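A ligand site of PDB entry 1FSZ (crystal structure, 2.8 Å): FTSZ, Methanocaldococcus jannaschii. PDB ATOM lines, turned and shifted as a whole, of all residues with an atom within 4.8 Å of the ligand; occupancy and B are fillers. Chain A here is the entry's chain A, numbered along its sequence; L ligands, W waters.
Water W1 bridges N4 of the ligand (2.6 Å) and OD1 of Asn 192 (3.2 Å).
Water W5 bridges OE1 of Gln 75 and O2 of the ligand.
Water W3 lies within hydrogen-bond range of the backbone carbonyl oxygen of Gly 130 (2.7 Å), the backbone NH of Gly 133 (2.8 Å), an oxygen (O1) of the ligand (2.8 Å) and the side-chain hydroxyl of Thr 137 (3.0 Å).
Water W2 lies within hydrogen-bond range of the backbone carbonyl oxygen of Cys 45, the backbone NH of Gly 130, an oxygen (O5) of the ligand and the backbone NH of Gly 49.
Water W4 bridges O of Leu 131 (2.9 Å) and O10 of the ligand (3.2 Å).
Water W6 bridges NH2 of Arg 169 and O3 of the ligand.
Residues that only touch the ligand: Gly 46 (3.6 Å), Gly 130 (3.1 Å), Leu 131 (3.9 Å), Gly 133 (3.5 Å), Pro 161 (3.7 Å), Phe 208 (3.4 Å), Ala 211 (3.5 Å) and Leu 215 (3.95 Å).
Hydrophobic or aromatic side chains within 4 Å of the ligand: Ala 48, Pro 161, Phe 208, Ala 211 and Leu 215.
Within 4 Å of the ligand: Gly 46, Gly 47, Ala 48, Asn 51, Gly 130, Leu 131, Gly 133, Gly 134, Thr 135, Gly 136, Pro 161, Glu 165, Arg 169, Phe 208, Ala 211, Asp 212 and Leu 215.
The nearest printed residue that does not touch the ligand is Gly 132 (4.2 Å).
The side-chain carboxylate (OE1) of Glu 165 lies within salt-bridge range of the guanidinium group (NH1) of Arg 169 (3.7 Å).
OE2 of Glu 165 is in hydrogen-bond range of N of Phe 162, 2.9 Å away.
The side-chain carboxylate (OD2) of Asp 212 lies within hydrogen-bond range of the side-chain amide nitrogen (ND2) of Asn 51 (3.2 Å).
The side-chain amide nitrogen (NE2) of Gln 75 lies close to the backbone NH (N) of Gly 47.
The backbone carbonyl oxygen of Gly 133 is in hydrogen-bond range of the side-chain hydroxyl of Thr 137 (2.8 Å).
OE2 of Glu 165 is in hydrogen-bond range of O10 of the ligand, at 2.4 Å.
N3 of the ligand is in hydrogen-bond range of OD1 of Asp 212.
An oxygen (O5) of the ligand lies within hydrogen-bond range of the backbone NH (N) of Ala 48 (2.7 Å).
The guanidinium group (NH1) of Arg 169 is in hydrogen-bond range of an oxygen (O9) of the ligand.
The backbone NH (N) of Gly 136 lies within hydrogen-bond range of an oxygen (O1) of the ligand (2.9 Å).
An oxygen (O2) of the ligand lies within hydrogen-bond range of the backbone NH (N) of Gly 47 (2.9 Å).
N of Gly 134 lies within hydrogen-bond range of O3 of the ligand, at 3.1 Å.
An oxygen (O1) of the ligand is in hydrogen-bond range of the backbone NH (N) of Thr 135, at 3.3 Å.
The side-chain amide nitrogen (ND2) of Asn 51 lies within hydrogen-bond range of an oxygen (O11) of the ligand, 3.4 Å away.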
ATOM      1  N   CYS A  45      29.245 -16.285  -4.438  1.00  0.00           N
ATOM      2  CA  CYS A  45      30.578 -16.489  -5.022  1.00  0.00           C
ATOM      3  C   CYS A  45      30.673 -17.607  -6.054  1.00  0.00           C
ATOM      4  O   CYS A  45      30.155 -18.718  -5.837  1.00  0.00           O
ATOM      5  CB  CYS A  45      31.621 -16.726  -3.938  1.00  0.00           C
ATOM      6  SG  CYS A  45      31.498 -15.577  -2.563  1.00  0.00           S
ATOM      7  N   GLY A  46      31.365 -17.297  -7.164  1.00  0.00           N
ATOM      8  CA  GLY A  46      31.524 -18.249  -8.230  1.00  0.00           C
ATOM      9  C   GLY A  46      30.247 -18.376  -9.067  1.00  0.00           C
ATOM     10  O   GLY A  46      29.266 -17.655  -8.819  1.00  0.00           O
ATOM     11  N   GLY A  47      30.255 -19.272 -10.048  1.00  0.00           N
ATOM     12  CA  GLY A  47      29.094 -19.462 -10.906  1.00  0.00           C
ATOM     13  C   GLY A  47      27.778 -19.756 -10.200  1.00  0.00           C
ATOM     14  O   GLY A  47      26.793 -19.075 -10.422  1.00  0.00           O
ATOM     15  N   ALA A  48      27.751 -20.773  -9.347  1.00  0.00           N
ATOM     16  CA  ALA A  48      26.526 -21.116  -8.643  1.00  0.00           C
ATOM     17  C   ALA A  48      26.071 -19.975  -7.735  1.00  0.00           C
ATOM     18  O   ALA A  48      24.898 -19.634  -7.681  1.00  0.00           O
ATOM     19  CB  ALA A  48      26.730 -22.361  -7.839  1.00  0.00           C
ATOM     20  N   GLY A  49      27.015 -19.399  -6.994  1.00  0.00           N
ATOM     21  CA  GLY A  49      26.687 -18.310  -6.112  1.00  0.00           C
ATOM     22  C   GLY A  49      26.192 -17.128  -6.908  1.00  0.00           C
ATOM     23  O   GLY A  49      25.254 -16.449  -6.458  1.00  0.00           O
ATOM     24  N   ASN A  51      24.819 -17.329  -9.792  1.00  0.00           N
ATOM     25  CA  ASN A  51      23.549 -17.769 -10.308  1.00  0.00           C
ATOM     26  C   ASN A  51      22.456 -17.506  -9.298  1.00  0.00           C
ATOM     27  O   ASN A  51      21.351 -17.083  -9.653  1.00  0.00           O
ATOM     28  CB  ASN A  51      23.602 -19.262 -10.644  1.00  0.00           C
ATOM     29  CG  ASN A  51      22.328 -19.752 -11.325  1.00  0.00           C
ATOM     30  OD1 ASN A  51      21.644 -18.985 -12.026  1.00  0.00           O
ATOM     31  ND2 ASN A  51      22.003 -21.030 -11.118  1.00  0.00           N
ATOM     32  N   GLN A  75      30.849 -14.976 -16.634  1.00  0.00           N
ATOM     33  CA  GLN A  75      29.742 -15.336 -15.735  1.00  0.00           C
ATOM     34  C   GLN A  75      29.307 -14.110 -14.991  1.00  0.00           C
ATOM     35  O   GLN A  75      28.116 -13.861 -14.786  1.00  0.00           O
ATOM     36  CB  GLN A  75      30.179 -16.403 -14.720  1.00  0.00           C
ATOM     37  CG  GLN A  75      30.557 -17.721 -15.322  1.00  0.00           C
ATOM     38  CD  GLN A  75      30.877 -18.766 -14.286  1.00  0.00           C
ATOM     39  OE1 GLN A  75      30.867 -19.963 -14.577  1.00  0.00           O
ATOM     40  NE2 GLN A  75      31.172 -18.325 -13.080  1.00  0.00           N
ATOM     41  N   GLY A  99      38.464 -24.405 -11.331  1.00  0.00           N
ATOM     42  CA  GLY A  99      38.147 -25.418 -10.335  1.00  0.00           C
ATOM     43  C   GLY A  99      39.073 -25.485  -9.126  1.00  0.00           C
ATOM     44  O   GLY A  99      38.890 -26.320  -8.239  1.00  0.00           O
ATOM     45  N   GLY A 130      28.276 -22.612  -4.175  1.00  0.00           N
ATOM     46  CA  GLY A 130      28.256 -24.065  -4.283  1.00  0.00           C
ATOM     47  C   GLY A 130      29.676 -24.531  -4.002  1.00  0.00           C
ATOM     48  O   GLY A 130      30.573 -24.275  -4.810  1.00  0.00           O
ATOM     49  N   LEU A 131      29.901 -25.202  -2.864  1.00  0.00           N
ATOM     50  CA  LEU A 131      31.260 -25.661  -2.500  1.00  0.00           C
ATOM     51  C   LEU A 131      31.699 -26.807  -3.424  1.00  0.00           C
ATOM     52  O   LEU A 131      30.907 -27.697  -3.714  1.00  0.00           O
ATOM     53  CB  LEU A 131      31.301 -26.117  -1.028  1.00  0.00           C
ATOM     54  CG  LEU A 131      31.166 -25.093   0.118  1.00  0.00           C
ATOM     55  CD1 LEU A 131      31.414 -25.748   1.468  1.00  0.00           C
ATOM     56  CD2 LEU A 131      32.126 -23.928  -0.094  1.00  0.00           C
ATOM     57  N   GLY A 132      32.946 -26.792  -3.872  1.00  0.00           N
ATOM     58  CA  GLY A 132      33.449 -27.835  -4.752  1.00  0.00           C
ATOM     59  C   GLY A 132      34.243 -27.250  -5.910  1.00  0.00           C
ATOM     60  O   GLY A 132      35.123 -27.912  -6.464  1.00  0.00           O
ATOM     61  N   GLY A 133      33.926 -26.022  -6.277  1.00  0.00           N
ATOM     62  CA  GLY A 133      34.630 -25.349  -7.347  1.00  0.00           C
ATOM     63  C   GLY A 133      35.881 -24.636  -6.845  1.00  0.00           C
ATOM     64  O   GLY A 133      36.426 -25.031  -5.809  1.00  0.00           O
ATOM     65  N   GLY A 134      36.335 -23.594  -7.544  1.00  0.00           N
ATOM     66  CA  GLY A 134      37.532 -22.893  -7.122  1.00  0.00           C
ATOM     67  C   GLY A 134      37.259 -21.486  -6.608  1.00  0.00           C
ATOM     68  O   GLY A 134      37.777 -21.116  -5.569  1.00  0.00           O
ATOM     69  N   THR A 135      36.453 -20.700  -7.312  1.00  0.00           N
ATOM     70  CA  THR A 135      36.114 -19.358  -6.874  1.00  0.00           C
ATOM     71  C   THR A 135      35.312 -19.374  -5.561  1.00  0.00           C
ATOM     72  O   THR A 135      35.728 -18.762  -4.587  1.00  0.00           O
ATOM     73  CB  THR A 135      35.312 -18.637  -7.957  1.00  0.00           C
ATOM     74  OG1 THR A 135      36.089 -18.611  -9.157  1.00  0.00           O
ATOM     75  CG2 THR A 135      34.966 -17.210  -7.562  1.00  0.00           C
ATOM     76  N   GLY A 136      34.185 -20.088  -5.543  1.00  0.00           N
ATOM     77  CA  GLY A 136      33.375 -20.179  -4.337  1.00  0.00           C
ATOM     78  C   GLY A 136      34.119 -20.820  -3.172  1.00  0.00           C
ATOM     79  O   GLY A 136      34.323 -20.225  -2.126  1.00  0.00           O
ATOM     80  N   THR A 137      34.542 -22.055  -3.346  1.00  0.00           N
ATOM     81  CA  THR A 137      35.260 -22.720  -2.289  1.00  0.00           C
ATOM     82  C   THR A 137      36.449 -21.918  -1.777  1.00  0.00           C
ATOM     83  O   THR A 137      36.751 -21.961  -0.618  1.00  0.00           O
ATOM     84  CB  THR A 137      35.772 -24.047  -2.765  1.00  0.00           C
ATOM     85  OG1 THR A 137      34.754 -24.657  -3.544  1.00  0.00           O
ATOM     86  CG2 THR A 137      36.119 -24.938  -1.605  1.00  0.00           C
ATOM     87  N   PRO A 161      28.730 -30.628  -2.976  1.00  0.00           N
ATOM     88  CA  PRO A 161      28.450 -31.252  -4.272  1.00  0.00           C
ATOM     89  C   PRO A 161      27.721 -32.600  -4.237  1.00  0.00           C
ATOM     90  O   PRO A 161      27.726 -33.309  -3.216  1.00  0.00           O
ATOM     91  CB  PRO A 161      29.834 -31.384  -4.888  1.00  0.00           C
ATOM     92  CG  PRO A 161      30.752 -31.499  -3.694  1.00  0.00           C
ATOM     93  CD  PRO A 161      30.181 -30.508  -2.749  1.00  0.00           C
ATOM     94  N   PHE A 162      27.081 -32.950  -5.363  1.00  0.00           N
ATOM     95  CA  PHE A 162      26.387 -34.217  -5.510  1.00  0.00           C
ATOM     96  C   PHE A 162      27.483 -35.290  -5.550  1.00  0.00           C
ATOM     97  O   PHE A 162      28.588 -35.016  -6.015  1.00  0.00           O
ATOM     98  CB  PHE A 162      25.638 -34.249  -6.831  1.00  0.00           C
ATOM     99  CG  PHE A 162      24.373 -33.434  -6.850  1.00  0.00           C
ATOM    100  CD1 PHE A 162      23.211 -33.912  -6.253  1.00  0.00           C
ATOM    101  CD2 PHE A 162      24.308 -32.244  -7.550  1.00  0.00           C
ATOM    102  CE1 PHE A 162      21.995 -33.215  -6.368  1.00  0.00           C
ATOM    103  CE2 PHE A 162      23.114 -31.555  -7.671  1.00  0.00           C
ATOM    104  CZ  PHE A 162      21.952 -32.042  -7.077  1.00  0.00           C
ATOM    105  N   GLU A 165      29.450 -35.866  -8.917  1.00  0.00           N
ATOM    106  CA  GLU A 165      30.563 -34.974  -9.252  1.00  0.00           C
ATOM    107  C   GLU A 165      31.947 -35.527  -8.918  1.00  0.00           C
ATOM    108  O   GLU A 165      32.971 -34.995  -9.353  1.00  0.00           O
ATOM    109  CB  GLU A 165      30.350 -33.643  -8.563  1.00  0.00           C
ATOM    110  CG  GLU A 165      28.964 -33.076  -8.797  1.00  0.00           C
ATOM    111  CD  GLU A 165      28.819 -31.639  -8.339  1.00  0.00           C
ATOM    112  OE1 GLU A 165      29.628 -30.801  -8.742  1.00  0.00           O
ATOM    113  OE2 GLU A 165      27.879 -31.344  -7.581  1.00  0.00           O
ATOM    114  N   ARG A 169      35.910 -33.120  -6.263  1.00  0.00           N
ATOM    115  CA  ARG A 169      35.006 -32.020  -6.030  1.00  0.00           C
ATOM    116  C   ARG A 169      34.602 -31.960  -4.567  1.00  0.00           C
ATOM    117  O   ARG A 169      34.533 -30.883  -3.998  1.00  0.00           O
ATOM    118  CB  ARG A 169      33.760 -32.135  -6.909  1.00  0.00           C
ATOM    119  CG  ARG A 169      33.433 -30.912  -7.759  1.00  0.00           C
ATOM    120  CD  ARG A 169      34.293 -30.921  -9.012  1.00  0.00           C
ATOM    121  NE  ARG A 169      34.602 -29.607  -9.586  1.00  0.00           N
ATOM    122  CZ  ARG A 169      33.817 -28.533  -9.513  1.00  0.00           C
ATOM    123  NH1 ARG A 169      32.640 -28.583  -8.886  1.00  0.00           N
ATOM    124  NH2 ARG A 169      34.200 -27.396 -10.075  1.00  0.00           N
ATOM    125  N   ASN A 192      23.739 -31.472  -1.314  1.00  0.00           N
ATOM    126  CA  ASN A 192      22.916 -31.733  -2.483  1.00  0.00           C
ATOM    127  C   ASN A 192      22.567 -33.215  -2.637  1.00  0.00           C
ATOM    128  O   ASN A 192      21.495 -33.547  -3.149  1.00  0.00           O
ATOM    129  CB  ASN A 192      23.607 -31.189  -3.731  1.00  0.00           C
ATOM    130  CG  ASN A 192      23.409 -29.698  -3.868  1.00  0.00           C
ATOM    131  OD1 ASN A 192      24.011 -29.055  -4.726  1.00  0.00           O
ATOM    132  ND2 ASN A 192      22.569 -29.134  -3.021  1.00  0.00           N
ATOM    133  N   PHE A 208      20.461 -29.966 -10.469  1.00  0.00           N
ATOM    134  CA  PHE A 208      20.863 -28.595 -10.205  1.00  0.00           C
ATOM    135  C   PHE A 208      19.728 -27.580 -10.222  1.00  0.00           C
ATOM    136  O   PHE A 208      19.910 -26.434  -9.840  1.00  0.00           O
ATOM    137  CB  PHE A 208      21.960 -28.162 -11.182  1.00  0.00           C
ATOM    138  CG  PHE A 208      23.254 -28.863 -10.964  1.00  0.00           C
ATOM    139  CD1 PHE A 208      24.045 -28.550  -9.875  1.00  0.00           C
ATOM    140  CD2 PHE A 208      23.680 -29.863 -11.819  1.00  0.00           C
ATOM    141  CE1 PHE A 208      25.224 -29.227  -9.647  1.00  0.00           C
ATOM    142  CE2 PHE A 208      24.862 -30.547 -11.603  1.00  0.00           C
ATOM    143  CZ  PHE A 208      25.634 -30.224 -10.515  1.00  0.00           C
ATOM    144  N   ALA A 211      18.369 -28.147  -6.575  1.00  0.00           N
ATOM    145  CA  ALA A 211      19.353 -27.534  -5.697  1.00  0.00           C
ATOM    146  C   ALA A 211      19.225 -26.024  -5.779  1.00  0.00           C
ATOM    147  O   ALA A 211      19.350 -25.325  -4.778  1.00  0.00           O
ATOM    148  CB  ALA A 211      20.754 -27.968  -6.072  1.00  0.00           C
ATOM    149  N   ASP A 212      18.958 -25.512  -6.982  1.00  0.00           N
ATOM    150  CA  ASP A 212      18.788 -24.081  -7.161  1.00  0.00           C
ATOM    151  C   ASP A 212      17.613 -23.625  -6.298  1.00  0.00           C
ATOM    152  O   ASP A 212      17.672 -22.602  -5.628  1.00  0.00           O
ATOM    153  CB  ASP A 212      18.474 -23.771  -8.623  1.00  0.00           C
ATOM    154  CG  ASP A 212      19.690 -23.354  -9.415  1.00  0.00           C
ATOM    155  OD1 ASP A 212      20.826 -23.499  -8.933  1.00  0.00           O
ATOM    156  OD2 ASP A 212      19.489 -22.880 -10.548  1.00  0.00           O
ATOM    157  N   LEU A 215      18.291 -23.804  -2.431  1.00  0.00           N
ATOM    158  CA  LEU A 215      19.155 -22.671  -2.109  1.00  0.00           C
ATOM    159  C   LEU A 215      18.425 -21.353  -1.976  1.00  0.00           C
ATOM    160  O   LEU A 215      18.478 -20.729  -0.938  1.00  0.00           O
ATOM    161  CB  LEU A 215      20.253 -22.516  -3.174  1.00  0.00           C
ATOM    162  CG  LEU A 215      21.658 -22.941  -2.735  1.00  0.00           C
ATOM    163  CD1 LEU A 215      22.610 -22.949  -3.944  1.00  0.00           C
ATOM    164  CD2 LEU A 215      22.130 -21.997  -1.645  1.00  0.00           C
HETATM  165  P1  LIG L   1      33.057 -22.097  -9.187  1.00  0.00           P
HETATM  166  O1  LIG L   1      33.334 -21.639  -7.852  1.00  0.00           O
HETATM  167  O2  LIG L   1      32.468 -21.176 -10.141  1.00  0.00           O
HETATM  168  O3  LIG L   1      34.341 -22.765  -9.751  1.00  0.00           O
HETATM  169  O4  LIG L   1      32.056 -23.314  -8.979  1.00  0.00           O
HETATM  170  P2  LIG L   1      30.609 -23.558  -9.633  1.00  0.00           P
HETATM  171  O5  LIG L   1      29.622 -22.665  -8.988  1.00  0.00           O
HETATM  172  O6  LIG L   1      30.736 -23.606 -11.097  1.00  0.00           O
HETATM  173  O7  LIG L   1      30.381 -25.050  -9.079  1.00  0.00           O
HETATM  174  C1  LIG L   1      30.692 -25.370  -7.737  1.00  0.00           C
HETATM  175  C2  LIG L   1      29.705 -26.382  -7.171  1.00  0.00           C
HETATM  176  O8  LIG L   1      28.407 -25.804  -7.125  1.00  0.00           O
HETATM  177  C3  LIG L   1      29.555 -27.684  -7.972  1.00  0.00           C
HETATM  178  O9  LIG L   1      30.374 -28.713  -7.439  1.00  0.00           O
HETATM  179  C4  LIG L   1      28.066 -27.999  -8.018  1.00  0.00           C
HETATM  180  O10 LIG L   1      27.645 -28.974  -7.100  1.00  0.00           O
HETATM  181  C5  LIG L   1      27.443 -26.668  -7.727  1.00  0.00           C
HETATM  182  N1  LIG L   1      26.825 -26.039  -8.908  1.00  0.00           N
HETATM  183  C6  LIG L   1      27.284 -25.748 -10.165  1.00  0.00           C
HETATM  184  N2  LIG L   1      26.431 -25.178 -10.961  1.00  0.00           N
HETATM  185  C7  LIG L   1      25.284 -25.083 -10.181  1.00  0.00           C
HETATM  186  C8  LIG L   1      23.993 -24.547 -10.476  1.00  0.00           C
HETATM  187  O11 LIG L   1      23.616 -24.052 -11.517  1.00  0.00           O
HETATM  188  N3  LIG L   1      23.104 -24.643  -9.376  1.00  0.00           N
HETATM  189  C9  LIG L   1      23.431 -25.187  -8.125  1.00  0.00           C
HETATM  190  N4  LIG L   1      22.510 -25.210  -7.184  1.00  0.00           N
HETATM  191  N5  LIG L   1      24.626 -25.697  -7.857  1.00  0.00           N
HETATM  192  C10 LIG L   1      25.515 -25.602  -8.915  1.00  0.00           C
HETATM  193  O   HOH W   1      23.935 -25.905  -5.121  1.00  0.00           O
HETATM  194  O   HOH W   2      29.507 -21.176  -6.291  1.00  0.00           O
HETATM  195  O   HOH W   3      33.030 -23.438  -5.664  1.00  0.00           O
HETATM  196  O   HOH W   4      28.080 -27.730  -4.199  1.00  0.00           O
HETATM  197  O   HOH W   5      32.009 -21.748 -12.810  1.00  0.00           O
HETATM  198  O   HOH W   6      34.927 -25.129 -11.946  1.00  0.00           O
